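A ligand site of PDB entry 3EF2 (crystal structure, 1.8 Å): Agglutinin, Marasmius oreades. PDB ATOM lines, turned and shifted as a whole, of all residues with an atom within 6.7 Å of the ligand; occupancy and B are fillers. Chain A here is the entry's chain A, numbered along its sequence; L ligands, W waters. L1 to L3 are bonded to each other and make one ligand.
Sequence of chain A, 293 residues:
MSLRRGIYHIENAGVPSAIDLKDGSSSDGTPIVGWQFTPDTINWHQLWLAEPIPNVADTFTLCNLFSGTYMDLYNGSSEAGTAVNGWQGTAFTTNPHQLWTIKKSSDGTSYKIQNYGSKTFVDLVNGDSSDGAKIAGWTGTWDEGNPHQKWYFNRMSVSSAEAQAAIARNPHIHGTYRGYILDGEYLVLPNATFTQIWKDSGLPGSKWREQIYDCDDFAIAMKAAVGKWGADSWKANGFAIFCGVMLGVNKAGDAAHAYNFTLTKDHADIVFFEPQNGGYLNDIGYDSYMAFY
An oxygen (O6) of LG2 L2 lies within hydrogen-bond range of the side-chain carboxylate of Asp 20, at 2.6 Å. The side-chain amide nitrogen (ND2) of Asn 43 lies within hydrogen-bond range of an oxygen (O1) of LG3 L3, 2.7 Å away. N of Thr 38 sits at hydrogen-bond distance from O2 of LG3 L3, 3.2 Å away. The side-chain hydroxyl (OG1) of Thr 38 is in hydrogen-bond range of an oxygen (O2) of LG3 L3 (2.7 Å). An oxygen (O6) of LG2 L2 is in hydrogen-bond range of the backbone NH (N) of Asp 23 (2.8 Å). O5 of LG3 L3 is in hydrogen-bond range of NE1 of Trp 35 (3.0 Å). A ring nitrogen (ND1) of His 45 sits at hydrogen-bond distance from an oxygen (O6) of LG2 L2 (3.0 Å). The backbone carbonyl oxygen (O) of Gln 36 is in hydrogen-bond range of an oxygen (O3) of LG3 L3, 3.3 Å away.
Water W2 bridges O5 of LG3 L3 (2.7 Å) and OD2 of Asp 131 (2.8 Å). Water W4 lies within hydrogen-bond range of an oxygen (O1) of LG3 L3, the backbone NH (N) of His 45 and the backbone NH (N) of Trp 44. Water W5 lies within hydrogen-bond range of OG1 of Thr 41 (2.7 Å), O2 of LG3 L3 (2.7 Å), O of Ile 42 (3.2 Å) and ND2 of Asn 43 (3.3 Å). Water W6 lies within hydrogen-bond range of O1 of LG3 L3, N of Trp 44 and O of Ile 42. Water W7 lies within hydrogen-bond range of the side-chain carboxylate of Asp 23 (2.8 Å) and an oxygen (O1) of LG2 L2 (3.4 Å).
Merely in contact with the ligand: Leu 21, Lys 22, Phe 37, Gln 46 and Trp 44. Hydrophobic or aromatic side chains within 4 Å of the ligand: Trp 35, Trp 44 and His 45. Of the 20 residues printed, 12 come within 4 Å of the ligand.
NE2 of Gln 46 lies within hydrogen-bond range of OD2 of Asp 20. O of Asp 20 lies within hydrogen-bond range of N of Val 33, 2.8 Å away. The side-chain amide oxygen of Asn 43 sits close to the backbone carbonyl oxygen of Thr 38. The side-chain amide oxygen (OD1) of Asn 43 lies within hydrogen-bond range of the side-chain hydroxyl (OG1) of Thr 41, 3.4 Å away. The backbone carbonyl oxygen (O) of Thr 38 is in hydrogen-bond range of the side-chain hydroxyl (OG1) of Thr 41 (2.8 Å). N of Leu 21 sits at hydrogen-bond distance from O of His 45. The side-chain carboxylate (OD2) of Asp 131 sits close to the side-chain amide oxygen (OE1) of Gln 36, at 2.9 Å. A ring nitrogen (NE2) of His 9 lies within hydrogen-bond range of the side-chain amide oxygen (OE1) of Gln 46 (2.8 Å).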
ATOM      1  N   HIS A   9     -18.482  17.551 -16.538  1.00  0.00           N
ATOM      2  CA  HIS A   9     -18.406  18.732 -17.411  1.00  0.00           C
ATOM      3  C   HIS A   9     -19.417  19.699 -16.776  1.00  0.00           C
ATOM      4  O   HIS A   9     -20.597  19.357 -16.664  1.00  0.00           O
ATOM      5  CB  HIS A   9     -18.845  18.365 -18.841  1.00  0.00           C
ATOM      6  CG  HIS A   9     -18.606  19.465 -19.828  1.00  0.00           C
ATOM      7  ND1 HIS A   9     -19.627  20.122 -20.488  1.00  0.00           N
ATOM      8  CD2 HIS A   9     -17.451  20.049 -20.255  1.00  0.00           C
ATOM      9  CE1 HIS A   9     -19.120  21.055 -21.269  1.00  0.00           C
ATOM     10  NE2 HIS A   9     -17.798  21.018 -21.163  1.00  0.00           N
ATOM     11  N   ASP A  20     -13.737  26.081 -17.490  1.00  0.00           N
ATOM     12  CA  ASP A  20     -12.613  25.750 -18.380  1.00  0.00           C
ATOM     13  C   ASP A  20     -11.326  26.226 -17.695  1.00  0.00           C
ATOM     14  O   ASP A  20     -11.230  27.400 -17.282  1.00  0.00           O
ATOM     15  CB  ASP A  20     -12.851  26.489 -19.719  1.00  0.00           C
ATOM     16  CG  ASP A  20     -11.787  26.193 -20.798  1.00  0.00           C
ATOM     17  OD1 ASP A  20     -10.606  26.531 -20.580  1.00  0.00           O
ATOM     18  OD2 ASP A  20     -12.150  25.645 -21.877  1.00  0.00           O
ATOM     19  N   LEU A  21     -10.343  25.338 -17.549  1.00  0.00           N
ATOM     20  CA  LEU A  21      -9.033  25.782 -17.091  1.00  0.00           C
ATOM     21  C   LEU A  21      -8.270  26.305 -18.296  1.00  0.00           C
ATOM     22  O   LEU A  21      -7.976  25.559 -19.246  1.00  0.00           O
ATOM     23  CB  LEU A  21      -8.279  24.638 -16.404  1.00  0.00           C
ATOM     24  CG  LEU A  21      -6.854  24.993 -15.949  1.00  0.00           C
ATOM     25  CD1 LEU A  21      -6.875  26.024 -14.807  1.00  0.00           C
ATOM     26  CD2 LEU A  21      -6.131  23.733 -15.494  1.00  0.00           C
ATOM     27  N   LYS A  22      -7.952  27.599 -18.275  1.00  0.00           N
ATOM     28  CA  LYS A  22      -7.527  28.291 -19.496  1.00  0.00           C
ATOM     29  C   LYS A  22      -6.265  27.662 -20.118  1.00  0.00           C
ATOM     30  O   LYS A  22      -5.229  27.539 -19.442  1.00  0.00           O
ATOM     31  CB  LYS A  22      -7.326  29.792 -19.257  1.00  0.00           C
ATOM     32  CG  LYS A  22      -7.301  30.603 -20.586  1.00  0.00           C
ATOM     33  CD  LYS A  22      -7.250  32.099 -20.357  1.00  0.00           C
ATOM     34  CE  LYS A  22      -7.498  32.830 -21.700  1.00  0.00           C
ATOM     35  NZ  LYS A  22      -7.624  34.330 -21.505  1.00  0.00           N
ATOM     36  N   ASP A  23      -6.378  27.262 -21.389  1.00  0.00           N
ATOM     37  CA  ASP A  23      -5.301  26.597 -22.158  1.00  0.00           C
ATOM     38  C   ASP A  23      -4.867  25.239 -21.540  1.00  0.00           C
ATOM     39  O   ASP A  23      -3.814  24.680 -21.902  1.00  0.00           O
ATOM     40  CB  ASP A  23      -4.070  27.517 -22.275  1.00  0.00           C
ATOM     41  CG  ASP A  23      -3.166  27.146 -23.457  1.00  0.00           C
ATOM     42  OD1 ASP A  23      -3.689  26.736 -24.511  1.00  0.00           O
ATOM     43  OD2 ASP A  23      -1.929  27.242 -23.319  1.00  0.00           O
ATOM     44  N   GLY A  24      -5.640  24.725 -20.591  1.00  0.00           N
ATOM     45  CA  GLY A  24      -5.282  23.497 -19.873  1.00  0.00           C
ATOM     46  C   GLY A  24      -3.973  23.621 -19.088  1.00  0.00           C
ATOM     47  O   GLY A  24      -3.375  22.597 -18.703  1.00  0.00           O
ATOM     48  N   VAL A  33     -12.145  29.883 -16.321  1.00  0.00           N
ATOM     49  CA  VAL A  33     -12.998  30.791 -17.109  1.00  0.00           C
ATOM     50  C   VAL A  33     -14.200  30.088 -17.741  1.00  0.00           C
ATOM     51  O   VAL A  33     -14.205  28.857 -17.917  1.00  0.00           O
ATOM     52  CB  VAL A  33     -12.174  31.472 -18.252  1.00  0.00           C
ATOM     53  CG1 VAL A  33     -11.057  32.389 -17.670  1.00  0.00           C
ATOM     54  CG2 VAL A  33     -11.571  30.412 -19.236  1.00  0.00           C
ATOM     55  N   TRP A  35     -16.237  29.082 -21.027  1.00  0.00           N
ATOM     56  CA  TRP A  35     -15.837  28.826 -22.411  1.00  0.00           C
ATOM     57  C   TRP A  35     -16.878  27.925 -23.098  1.00  0.00           C
ATOM     58  O   TRP A  35     -17.443  27.036 -22.474  1.00  0.00           O
ATOM     59  CB  TRP A  35     -14.433  28.192 -22.475  1.00  0.00           C
ATOM     60  CG  TRP A  35     -13.688  28.428 -23.765  1.00  0.00           C
ATOM     61  CD1 TRP A  35     -13.903  27.829 -24.981  1.00  0.00           C
ATOM     62  CD2 TRP A  35     -12.606  29.356 -23.955  1.00  0.00           C
ATOM     63  NE1 TRP A  35     -13.004  28.327 -25.914  1.00  0.00           N
ATOM     64  CE2 TRP A  35     -12.199  29.255 -25.304  1.00  0.00           C
ATOM     65  CE3 TRP A  35     -11.935  30.262 -23.100  1.00  0.00           C
ATOM     66  CZ2 TRP A  35     -11.158  30.051 -25.834  1.00  0.00           C
ATOM     67  CZ3 TRP A  35     -10.899  31.038 -23.622  1.00  0.00           C
ATOM     68  CH2 TRP A  35     -10.526  30.940 -24.988  1.00  0.00           C
ATOM     69  N   GLN A  36     -17.141  28.175 -24.378  1.00  0.00           N
ATOM     70  CA  GLN A  36     -18.080  27.355 -25.121  1.00  0.00           C
ATOM     71  C   GLN A  36     -17.538  25.925 -25.319  1.00  0.00           C
ATOM     72  O   GLN A  36     -16.345  25.698 -25.182  1.00  0.00           O
ATOM     73  CB  GLN A  36     -18.434  28.001 -26.475  1.00  0.00           C
ATOM     74  CG  GLN A  36     -17.272  28.062 -27.486  1.00  0.00           C
ATOM     75  CD  GLN A  36     -17.681  28.731 -28.782  1.00  0.00           C
ATOM     76  OE1 GLN A  36     -17.179  29.811 -29.143  1.00  0.00           O
ATOM     77  NE2 GLN A  36     -18.648  28.126 -29.465  1.00  0.00           N
ATOM     78  N   PHE A  37     -18.432  25.010 -25.671  1.00  0.00           N
ATOM     79  CA  PHE A  37     -18.124  23.584 -25.717  1.00  0.00           C
ATOM     80  C   PHE A  37     -18.853  22.900 -26.850  1.00  0.00           C
ATOM     81  O   PHE A  37     -19.807  23.456 -27.448  1.00  0.00           O
ATOM     82  CB  PHE A  37     -18.412  22.914 -24.343  1.00  0.00           C
ATOM     83  CG  PHE A  37     -19.864  22.960 -23.909  1.00  0.00           C
ATOM     84  CD1 PHE A  37     -20.732  21.919 -24.240  1.00  0.00           C
ATOM     85  CD2 PHE A  37     -20.344  24.012 -23.120  1.00  0.00           C
ATOM     86  CE1 PHE A  37     -22.082  21.947 -23.821  1.00  0.00           C
ATOM     87  CE2 PHE A  37     -21.688  24.060 -22.711  1.00  0.00           C
ATOM     88  CZ  PHE A  37     -22.544  23.017 -23.048  1.00  0.00           C
ATOM     89  N   THR A  38     -18.376  21.713 -27.175  1.00  0.00           N
ATOM     90  CA  THR A  38     -18.993  20.940 -28.238  1.00  0.00           C
ATOM     91  C   THR A  38     -19.506  19.653 -27.565  1.00  0.00           C
ATOM     92  O   THR A  38     -18.719  18.854 -27.042  1.00  0.00           O
ATOM     93  CB  THR A  38     -18.001  20.636 -29.393  1.00  0.00           C
ATOM     94  OG1 THR A  38     -17.354  21.852 -29.849  1.00  0.00           O
ATOM     95  CG2 THR A  38     -18.749  19.983 -30.572  1.00  0.00           C
ATOM     96  N   PRO A  39     -20.832  19.458 -27.556  1.00  0.00           N
ATOM     97  CA  PRO A  39     -21.381  18.224 -26.983  1.00  0.00           C
ATOM     98  C   PRO A  39     -20.880  17.000 -27.734  1.00  0.00           C
ATOM     99  O   PRO A  39     -20.561  17.099 -28.916  1.00  0.00           O
ATOM    100  CB  PRO A  39     -22.889  18.386 -27.187  1.00  0.00           C
ATOM    101  CG  PRO A  39     -23.109  19.889 -27.317  1.00  0.00           C
ATOM    102  CD  PRO A  39     -21.893  20.355 -28.062  1.00  0.00           C
ATOM    103  N   THR A  41     -18.105  15.382 -27.509  1.00  0.00           N
ATOM    104  CA  THR A  41     -16.661  15.353 -27.697  1.00  0.00           C
ATOM    105  C   THR A  41     -16.014  15.274 -26.324  1.00  0.00           C
ATOM    106  O   THR A  41     -16.699  15.476 -25.309  1.00  0.00           O
ATOM    107  CB  THR A  41     -16.107  16.633 -28.367  1.00  0.00           C
ATOM    108  OG1 THR A  41     -16.180  17.725 -27.449  1.00  0.00           O
ATOM    109  CG2 THR A  41     -16.859  16.970 -29.684  1.00  0.00           C
ATOM    110  N   ILE A  42     -14.723  14.991 -26.308  1.00  0.00           N
ATOM    111  CA  ILE A  42     -13.921  15.232 -25.136  1.00  0.00           C
ATOM    112  C   ILE A  42     -13.581  16.723 -25.171  1.00  0.00           C
ATOM    113  O   ILE A  42     -12.916  17.209 -26.088  1.00  0.00           O
ATOM    114  CB  ILE A  42     -12.617  14.375 -25.151  1.00  0.00           C
ATOM    115  CG1 ILE A  42     -12.965  12.868 -24.989  1.00  0.00           C
ATOM    116  CG2 ILE A  42     -11.632  14.865 -24.092  1.00  0.00           C
ATOM    117  CD1 ILE A  42     -13.682  12.455 -23.676  1.00  0.00           C
ATOM    118  N   ASN A  43     -14.084  17.445 -24.170  1.00  0.00           N
ATOM    119  CA  ASN A  43     -13.748  18.860 -24.005  1.00  0.00           C
ATOM    120  C   ASN A  43     -12.528  18.942 -23.101  1.00  0.00           C
ATOM    121  O   ASN A  43     -12.636  18.931 -21.873  1.00  0.00           O
ATOM    122  CB  ASN A  43     -14.939  19.639 -23.453  1.00  0.00           C
ATOM    123  CG  ASN A  43     -16.069  19.752 -24.452  1.00  0.00           C
ATOM    124  OD1 ASN A  43     -17.062  19.011 -24.387  1.00  0.00           O
ATOM    125  ND2 ASN A  43     -15.943  20.672 -25.395  1.00  0.00           N
ATOM    126  N   TRP A  44     -11.369  19.006 -23.758  1.00  0.00           N
ATOM    127  CA  TRP A  44     -10.061  18.700 -23.144  1.00  0.00           C
ATOM    128  C   TRP A  44      -9.726  19.496 -21.885  1.00  0.00           C
ATOM    129  O   TRP A  44      -9.073  18.977 -20.979  1.00  0.00           O
ATOM    130  CB  TRP A  44      -8.946  18.860 -24.193  1.00  0.00           C
ATOM    131  CG  TRP A  44      -8.885  17.688 -25.081  1.00  0.00           C
ATOM    132  CD1 TRP A  44      -9.511  17.507 -26.285  1.00  0.00           C
ATOM    133  CD2 TRP A  44      -8.208  16.456 -24.786  1.00  0.00           C
ATOM    134  NE1 TRP A  44      -9.244  16.242 -26.778  1.00  0.00           N
ATOM    135  CE2 TRP A  44      -8.444  15.584 -25.878  1.00  0.00           C
ATOM    136  CE3 TRP A  44      -7.417  16.024 -23.710  1.00  0.00           C
ATOM    137  CZ2 TRP A  44      -7.916  14.287 -25.917  1.00  0.00           C
ATOM    138  CZ3 TRP A  44      -6.894  14.734 -23.748  1.00  0.00           C
ATOM    139  CH2 TRP A  44      -7.136  13.886 -24.856  1.00  0.00           C
ATOM    140  N   HIS A  45     -10.179  20.747 -21.827  1.00  0.00           N
ATOM    141  CA  HIS A  45      -9.788  21.627 -20.716  1.00  0.00           C
ATOM    142  C   HIS A  45     -10.910  21.806 -19.689  1.00  0.00           C
ATOM    143  O   HIS A  45     -10.790  22.609 -18.760  1.00  0.00           O
ATOM    144  CB  HIS A  45      -9.349  22.997 -21.243  1.00  0.00           C
ATOM    145  CG  HIS A  45      -8.143  22.944 -22.139  1.00  0.00           C
ATOM    146  ND1 HIS A  45      -7.847  23.945 -23.035  1.00  0.00           N
ATOM    147  CD2 HIS A  45      -7.177  22.013 -22.277  1.00  0.00           C
ATOM    148  CE1 HIS A  45      -6.751  23.631 -23.703  1.00  0.00           C
ATOM    149  NE2 HIS A  45      -6.306  22.466 -23.240  1.00  0.00           N
ATOM    150  N   GLN A  46     -11.988  21.037 -19.876  1.00  0.00           N
ATOM    151  CA  GLN A  46     -13.246  21.280 -19.193  1.00  0.00           C
ATOM    152  C   GLN A  46     -13.770  20.069 -18.406  1.00  0.00           C
ATOM    153  O   GLN A  46     -14.963  20.011 -18.096  1.00  0.00           O
ATOM    154  CB  GLN A  46     -14.309  21.737 -20.197  1.00  0.00           C
ATOM    155  CG  GLN A  46     -13.916  22.980 -20.968  1.00  0.00           C
ATOM    156  CD  GLN A  46     -14.942  23.386 -22.025  1.00  0.00           C
ATOM    157  OE1 GLN A  46     -15.921  22.686 -22.286  1.00  0.00           O
ATOM    158  NE2 GLN A  46     -14.697  24.545 -22.643  1.00  0.00           N
ATOM    159  N   PHE A  66      -7.138  17.157 -17.289  1.00  0.00           N
ATOM    160  CA  PHE A  66      -5.997  17.385 -18.149  1.00  0.00           C
ATOM    161  C   PHE A  66      -4.760  17.888 -17.397  1.00  0.00           C
ATOM    162  O   PHE A  66      -3.671  17.341 -17.582  1.00  0.00           O
ATOM    163  CB  PHE A  66      -6.374  18.342 -19.285  1.00  0.00           C
ATOM    164  CG  PHE A  66      -5.240  18.604 -20.231  1.00  0.00           C
ATOM    165  CD1 PHE A  66      -4.852  17.644 -21.160  1.00  0.00           C
ATOM    166  CD2 PHE A  66      -4.543  19.801 -20.180  1.00  0.00           C
ATOM    167  CE1 PHE A  66      -3.784  17.880 -22.040  1.00  0.00           C
ATOM    168  CE2 PHE A  66      -3.472  20.049 -21.041  1.00  0.00           C
ATOM    169  CZ  PHE A  66      -3.107  19.096 -21.971  1.00  0.00           C
ATOM    170  N   ASP A 131     -16.072  33.511 -24.605  1.00  0.00           N
ATOM    171  CA  ASP A 131     -14.944  32.628 -24.316  1.00  0.00           C
ATOM    172  C   ASP A 131     -13.891  33.393 -23.538  1.00  0.00           C
ATOM    173  O   ASP A 131     -13.397  34.452 -23.971  1.00  0.00           O
ATOM    174  CB  ASP A 131     -14.344  32.076 -25.608  1.00  0.00           C
ATOM    175  CG  ASP A 131     -15.300  31.151 -26.359  1.00  0.00           C
ATOM    176  OD1 ASP A 131     -16.268  30.648 -25.729  1.00  0.00           O
ATOM    177  OD2 ASP A 131     -15.086  30.947 -27.572  1.00  0.00           O
HETATM  178  C1  LIG L   1      -9.864  22.897 -28.345  1.00  0.00           C
HETATM  179  C2  LIG L   1      -9.703  22.795 -29.876  1.00  0.00           C
HETATM  180  C3  LIG L   1      -8.210  22.679 -30.242  1.00  0.00           C
HETATM  181  C4  LIG L   1      -7.535  21.609 -29.368  1.00  0.00           C
HETATM  182  C5  LIG L   1      -7.752  21.906 -27.873  1.00  0.00           C
HETATM  183  C6  LIG L   1      -7.097  20.902 -26.948  1.00  0.00           C
HETATM  184  O1  LIG L   1     -10.260  23.934 -30.505  1.00  0.00           O
HETATM  185  O2  LIG L   1      -8.094  22.438 -31.638  1.00  0.00           O
HETATM  186  O3  LIG L   1      -8.036  20.313 -29.652  1.00  0.00           O
HETATM  187  O4  LIG L   1      -9.157  21.918 -27.620  1.00  0.00           O
HETATM  188  C1  LG2 L   2      -8.357  25.578 -26.398  1.00  0.00           C
HETATM  189  C2  LG2 L   2      -9.481  24.537 -26.587  1.00  0.00           C
HETATM  190  C3  LG2 L   2     -10.838  25.117 -26.216  1.00  0.00           C
HETATM  191  C4  LG2 L   2     -10.809  25.796 -24.837  1.00  0.00           C
HETATM  192  C5  LG2 L   2      -9.618  26.789 -24.800  1.00  0.00           C
HETATM  193  C6  LG2 L   2      -9.481  27.537 -23.464  1.00  0.00           C
HETATM  194  O1  LG2 L   2      -7.117  24.941 -26.546  1.00  0.00           O
HETATM  195  O2  LG2 L   2      -9.420  24.160 -27.914  1.00  0.00           O
HETATM  196  O3  LG2 L   2     -11.820  24.068 -26.282  1.00  0.00           O
HETATM  197  O4  LG2 L   2     -10.638  24.847 -23.825  1.00  0.00           O
HETATM  198  O5  LG2 L   2      -8.401  26.101 -25.075  1.00  0.00           O
HETATM  199  O6  LG2 L   2      -8.865  26.712 -22.474  1.00  0.00           O
HETATM  200  C1  LG3 L   3     -13.110  24.429 -26.145  1.00  0.00           C
HETATM  201  C2  LG3 L   3     -14.086  23.265 -26.358  1.00  0.00           C
HETATM  202  C3  LG3 L   3     -14.227  22.975 -27.868  1.00  0.00           C
HETATM  203  C4  LG3 L   3     -14.521  24.269 -28.664  1.00  0.00           C
HETATM  204  C5  LG3 L   3     -13.434  25.313 -28.360  1.00  0.00           C
HETATM  205  C6  LG3 L   3     -13.594  26.653 -29.078  1.00  0.00           C
HETATM  206  O1  LG3 L   3     -13.644  22.093 -25.632  1.00  0.00           O
HETATM  207  O2  LG3 L   3     -15.277  22.010 -28.074  1.00  0.00           O
HETATM  208  O3  LG3 L   3     -15.806  24.765 -28.285  1.00  0.00           O
HETATM  209  O4  LG3 L   3     -13.470  25.566 -26.953  1.00  0.00           O
HETATM  210  O5  LG3 L   3     -12.512  27.568 -28.734  1.00  0.00           O
HETATM  211  O   HOH W   1     -10.042  26.616 -29.743  1.00  0.00           O
HETATM  212  O   HOH W   2     -12.852  30.183 -29.057  1.00  0.00           O
HETATM  213  O   HOH W   3     -10.617  19.503 -29.139  1.00  0.00           O
HETATM  214  O   HOH W   4     -11.669  22.263 -23.732  1.00  0.00           O
HETATM  215  O   HOH W   5     -14.148  19.512 -27.913  1.00  0.00           O
HETATM  216  O   HOH W   6     -11.640  20.166 -26.564  1.00  0.00           O
HETATM  217  O   HOH W   7      -3.965  24.198 -25.625  1.00  0.00           O
HETATM  218  O   HOH W   8     -12.861  23.458 -31.348  1.00  0.00           O
